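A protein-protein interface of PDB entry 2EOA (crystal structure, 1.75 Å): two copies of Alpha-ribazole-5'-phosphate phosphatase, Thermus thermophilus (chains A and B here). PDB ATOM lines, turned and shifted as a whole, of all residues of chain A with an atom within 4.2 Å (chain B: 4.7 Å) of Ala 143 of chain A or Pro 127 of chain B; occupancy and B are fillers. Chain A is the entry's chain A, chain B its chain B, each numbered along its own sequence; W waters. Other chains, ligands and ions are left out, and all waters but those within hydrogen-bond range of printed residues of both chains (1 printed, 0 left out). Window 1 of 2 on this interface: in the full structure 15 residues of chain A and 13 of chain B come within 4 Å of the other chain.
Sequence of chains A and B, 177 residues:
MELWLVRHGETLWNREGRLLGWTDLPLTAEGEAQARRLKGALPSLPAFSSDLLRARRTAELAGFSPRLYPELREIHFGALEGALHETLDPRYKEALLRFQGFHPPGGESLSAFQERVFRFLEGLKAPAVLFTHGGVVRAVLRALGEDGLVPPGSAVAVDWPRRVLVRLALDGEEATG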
ATOM      1  N   PHE A 118     -19.429  11.787  -3.093  1.00  0.00           N
ATOM      2  CA  PHE A 118     -18.863  12.877  -3.881  1.00  0.00           C
ATOM      3  C   PHE A 118     -19.782  13.363  -4.999  1.00  0.00           C
ATOM      4  O   PHE A 118     -19.754  14.542  -5.356  1.00  0.00           O
ATOM      5  CB  PHE A 118     -17.497  12.471  -4.431  1.00  0.00           C
ATOM      6  CG  PHE A 118     -16.509  12.099  -3.358  1.00  0.00           C
ATOM      7  CD1 PHE A 118     -16.522  12.754  -2.126  1.00  0.00           C
ATOM      8  CD2 PHE A 118     -15.560  11.110  -3.576  1.00  0.00           C
ATOM      9  CE1 PHE A 118     -15.595  12.424  -1.124  1.00  0.00           C
ATOM     10  CE2 PHE A 118     -14.629  10.773  -2.582  1.00  0.00           C
ATOM     11  CZ  PHE A 118     -14.651  11.433  -1.356  1.00  0.00           C
ATOM     12  N   ALA A 139     -14.661  10.317   4.730  1.00  0.00           N
ATOM     13  CA  ALA A 139     -14.335  10.278   3.307  1.00  0.00           C
ATOM     14  C   ALA A 139     -13.971  11.674   2.803  1.00  0.00           C
ATOM     15  O   ALA A 139     -13.024  11.848   2.043  1.00  0.00           O
ATOM     16  CB  ALA A 139     -15.530   9.726   2.511  1.00  0.00           C
ATOM     17  N   VAL A 140     -14.737  12.666   3.241  1.00  0.00           N
ATOM     18  CA  VAL A 140     -14.507  14.048   2.836  1.00  0.00           C
ATOM     19  C   VAL A 140     -13.189  14.583   3.390  1.00  0.00           C
ATOM     20  O   VAL A 140     -12.383  15.153   2.651  1.00  0.00           O
ATOM     21  CB  VAL A 140     -15.672  14.949   3.312  1.00  0.00           C
ATOM     22  CG1 VAL A 140     -15.342  16.426   3.076  1.00  0.00           C
ATOM     23  CG2 VAL A 140     -16.946  14.571   2.561  1.00  0.00           C
ATOM     24  N   LEU A 141     -12.970  14.400   4.689  1.00  0.00           N
ATOM     25  CA  LEU A 141     -11.739  14.884   5.309  1.00  0.00           C
ATOM     26  C   LEU A 141     -10.517  14.195   4.709  1.00  0.00           C
ATOM     27  O   LEU A 141      -9.505  14.845   4.424  1.00  0.00           O
ATOM     28  CB  LEU A 141     -11.775  14.665   6.827  1.00  0.00           C
ATOM     29  CG  LEU A 141     -12.797  15.521   7.586  1.00  0.00           C
ATOM     30  CD1 LEU A 141     -12.675  15.262   9.080  1.00  0.00           C
ATOM     31  CD2 LEU A 141     -12.568  16.996   7.283  1.00  0.00           C
ATOM     32  N   ARG A 142     -10.611  12.882   4.502  1.00  0.00           N
ATOM     33  CA  ARG A 142      -9.493  12.140   3.930  1.00  0.00           C
ATOM     34  C   ARG A 142      -9.187  12.595   2.504  1.00  0.00           C
ATOM     35  O   ARG A 142      -8.024  12.679   2.109  1.00  0.00           O
ATOM     36  CB  ARG A 142      -9.770  10.633   3.934  1.00  0.00           C
ATOM     37  CG  ARG A 142      -9.655   9.967   5.297  1.00  0.00           C
ATOM     38  CD  ARG A 142      -9.777   8.450   5.186  1.00  0.00           C
ATOM     39  NE  ARG A 142      -8.657   7.844   4.464  1.00  0.00           N
ATOM     40  CZ  ARG A 142      -7.543   7.395   5.043  1.00  0.00           C
ATOM     41  NH1 ARG A 142      -7.386   7.477   6.359  1.00  0.00           N
ATOM     42  NH2 ARG A 142      -6.586   6.849   4.304  1.00  0.00           N
ATOM     43  N   ALA A 143     -10.229  12.891   1.734  1.00  0.00           N
ATOM     44  CA  ALA A 143     -10.033  13.338   0.358  1.00  0.00           C
ATOM     45  C   ALA A 143      -9.339  14.698   0.362  1.00  0.00           C
ATOM     46  O   ALA A 143      -8.662  15.065  -0.597  1.00  0.00           O
ATOM     47  CB  ALA A 143     -11.374  13.433  -0.363  1.00  0.00           C
ATOM     48  N   LEU A 144      -9.509  15.439   1.449  1.00  0.00           N
ATOM     49  CA  LEU A 144      -8.891  16.754   1.571  1.00  0.00           C
ATOM     50  C   LEU A 144      -7.526  16.634   2.239  1.00  0.00           C
ATOM     51  O   LEU A 144      -6.924  17.630   2.652  1.00  0.00           O
ATOM     52  CB  LEU A 144      -9.811  17.703   2.348  1.00  0.00           C
ATOM     53  CG  LEU A 144     -11.139  18.000   1.633  1.00  0.00           C
ATOM     54  CD1 LEU A 144     -12.005  18.921   2.491  1.00  0.00           C
ATOM     55  CD2 LEU A 144     -10.868  18.644   0.271  1.00  0.00           C
ATOM     56  N   GLY A 145      -7.053  15.396   2.338  1.00  0.00           N
ATOM     57  CA  GLY A 145      -5.742  15.119   2.901  1.00  0.00           C
ATOM     58  C   GLY A 145      -5.550  15.218   4.402  1.00  0.00           C
ATOM     59  O   GLY A 145      -4.419  15.408   4.857  1.00  0.00           O
ATOM     60  N   PRO A 161     -14.083  21.478  -3.334  1.00  0.00           N
ATOM     61  CA  PRO A 161     -13.248  20.335  -2.943  1.00  0.00           C
ATOM     62  C   PRO A 161     -11.790  20.759  -2.757  1.00  0.00           C
ATOM     63  O   PRO A 161     -10.876  20.106  -3.267  1.00  0.00           O
ATOM     64  CB  PRO A 161     -13.389  19.419  -4.140  1.00  0.00           C
ATOM     65  CG  PRO A 161     -13.245  20.417  -5.275  1.00  0.00           C
ATOM     66  CD  PRO A 161     -14.073  21.630  -4.804  1.00  0.00           C
ATOM     67  N   MET B   1      -8.634  21.672  -7.644  1.00  0.00           N
ATOM     68  CA  MET B   1      -8.767  20.366  -6.932  1.00  0.00           C
ATOM     69  C   MET B   1      -7.476  19.559  -7.071  1.00  0.00           C
ATOM     70  O   MET B   1      -6.986  19.329  -8.178  1.00  0.00           O
ATOM     71  CB  MET B   1      -9.948  19.585  -7.506  1.00  0.00           C
ATOM     72  CG  MET B   1     -10.335  18.378  -6.683  1.00  0.00           C
ATOM     73  SD  MET B   1     -11.893  17.696  -7.231  1.00  0.00           S
ATOM     74  CE  MET B   1     -11.384  16.802  -8.701  1.00  0.00           C
ATOM     75  N   GLU B   2      -6.941  19.125  -5.935  1.00  0.00           N
ATOM     76  CA  GLU B   2      -5.687  18.387  -5.899  1.00  0.00           C
ATOM     77  C   GLU B   2      -5.697  17.014  -6.557  1.00  0.00           C
ATOM     78  O   GLU B   2      -6.475  16.140  -6.175  1.00  0.00           O
ATOM     79  CB  GLU B   2      -5.220  18.236  -4.451  1.00  0.00           C
ATOM     80  CG  GLU B   2      -3.802  17.703  -4.328  1.00  0.00           C
ATOM     81  CD  GLU B   2      -3.242  17.873  -2.934  1.00  0.00           C
ATOM     82  OE1 GLU B   2      -3.580  18.888  -2.290  1.00  0.00           O
ATOM     83  OE2 GLU B   2      -2.456  17.009  -2.488  1.00  0.00           O
ATOM     84  N   LEU B   3      -4.822  16.841  -7.544  1.00  0.00           N
ATOM     85  CA  LEU B   3      -4.682  15.565  -8.244  1.00  0.00           C
ATOM     86  C   LEU B   3      -3.207  15.197  -8.313  1.00  0.00           C
ATOM     87  O   LEU B   3      -2.360  16.028  -8.647  1.00  0.00           O
ATOM     88  CB  LEU B   3      -5.230  15.645  -9.675  1.00  0.00           C
ATOM     89  CG  LEU B   3      -6.690  16.041  -9.904  1.00  0.00           C
ATOM     90  CD1 LEU B   3      -6.963  16.032 -11.409  1.00  0.00           C
ATOM     91  CD2 LEU B   3      -7.635  15.078  -9.181  1.00  0.00           C
ATOM     92  N   LEU B  45      -5.361   9.598  -0.700  1.00  0.00           N
ATOM     93  CA  LEU B  45      -6.578  10.117  -1.312  1.00  0.00           C
ATOM     94  C   LEU B  45      -7.201   8.996  -2.139  1.00  0.00           C
ATOM     95  O   LEU B  45      -6.567   7.957  -2.358  1.00  0.00           O
ATOM     96  CB  LEU B  45      -6.241  11.276  -2.258  1.00  0.00           C
ATOM     97  CG  LEU B  45      -5.263  12.345  -1.763  1.00  0.00           C
ATOM     98  CD1 LEU B  45      -5.048  13.382  -2.853  1.00  0.00           C
ATOM     99  CD2 LEU B  45      -5.802  12.997  -0.504  1.00  0.00           C
ATOM    100  N   PRO B  46      -8.453   9.183  -2.597  1.00  0.00           N
ATOM    101  CA  PRO B  46      -9.093   8.145  -3.413  1.00  0.00           C
ATOM    102  C   PRO B  46      -8.148   7.855  -4.573  1.00  0.00           C
ATOM    103  O   PRO B  46      -7.566   8.783  -5.146  1.00  0.00           O
ATOM    104  CB  PRO B  46     -10.378   8.823  -3.880  1.00  0.00           C
ATOM    105  CG  PRO B  46     -10.734   9.677  -2.713  1.00  0.00           C
ATOM    106  CD  PRO B  46      -9.399  10.276  -2.303  1.00  0.00           C
ATOM    107  N   ALA B 126     -13.571  14.598  -6.677  1.00  0.00           N
ATOM    108  CA  ALA B 126     -12.845  14.808  -5.434  1.00  0.00           C
ATOM    109  C   ALA B 126     -11.361  14.612  -5.696  1.00  0.00           C
ATOM    110  O   ALA B 126     -10.982  14.040  -6.718  1.00  0.00           O
ATOM    111  CB  ALA B 126     -13.322  13.816  -4.369  1.00  0.00           C
ATOM    112  N   PRO B 127     -10.502  15.099  -4.783  1.00  0.00           N
ATOM    113  CA  PRO B 127      -9.054  14.946  -4.948  1.00  0.00           C
ATOM    114  C   PRO B 127      -8.748  13.468  -5.147  1.00  0.00           C
ATOM    115  O   PRO B 127      -9.498  12.606  -4.680  1.00  0.00           O
ATOM    116  CB  PRO B 127      -8.503  15.475  -3.632  1.00  0.00           C
ATOM    117  CG  PRO B 127      -9.465  16.574  -3.309  1.00  0.00           C
ATOM    118  CD  PRO B 127     -10.805  15.918  -3.596  1.00  0.00           C
ATOM    119  N   ALA B 128      -7.649  13.169  -5.828  1.00  0.00           N
ATOM    120  CA  ALA B 128      -7.313  11.781  -6.085  1.00  0.00           C
ATOM    121  C   ALA B 128      -5.860  11.566  -6.462  1.00  0.00           C
ATOM    122  O   ALA B 128      -5.142  12.508  -6.807  1.00  0.00           O
ATOM    123  CB  ALA B 128      -8.203  11.250  -7.204  1.00  0.00           C
HETATM  124  O   HOH W   1      -8.135  19.788  -3.507  1.00  0.00           O
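Printed residues of chain B that touch a printed residue of chain A: Met 1, Leu 45, Ala 126 and Pro 127. Hydrophobic or aromatic side chains of chain B that line the printed part of chain A: Met 1, Leu 45, Ala 126 and Pro 127. Among the printed residues, 7 pairs touch across the chains. Among the printed residues, no Asp or Glu carboxylate lies within 4 Å of a Lys or Arg side-chain nitrogen of the other chain.
Among the printed residues, pairs that only touch across the chains: Phe 118 of chain A with Ala 126 of chain B (3.6 Å), Arg 142 of chain A with Leu 45 of chain B (3.4 Å), Ala 143 of chain A with Leu 45 of chain B (3.5 Å), Ala 143 of chain A with Pro 127 of chain B (3.1 Å), Gly 145 of chain A with Leu 45 of chain B (3.9 Å), Pro 161 of chain A with Met 1 of chain B (3.6 Å) and Pro 161 of chain A with Pro 127 of chain B (3.8 Å).
No position is printed for both chains. Of the 7 pairs that touch across the chains among the printed residues, none has its exchanged pair printed and touching as well.
Ala 143 of chain A touches two residues of chain B. Pro 127 of chain B touches just these residues of chain A: Ala 143 (3.1 Å) and Pro 161 (3.8 Å). Printed residues of chain B within 4 Å of Gly 145 of chain A: Leu 45 (3.9 Å). Of the printed residues of chain A, Met 1 of chain B touches Pro 161 (3.6 Å). Printed residues of chain A within 4 Å of Ala 126 of chain B: Phe 118 (3.6 Å). Of the printed residues of chain A, Leu 45 of chain B touches Arg 142 (3.4 Å), Ala 143 (3.5 Å) and Gly 145 (3.9 Å). Ala 128 of chain B touches none of the printed residues of chain A.
The side-chain sulfur (SD) of Met 1 of chain B sits close to the backbone NH (N) of Ala 126 of chain B (3.6 Å).
Water W1 bridges the backbone carbonyl oxygen (O) of Pro 161 of chain A and the backbone NH (N) of Glu 2 of chain B.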
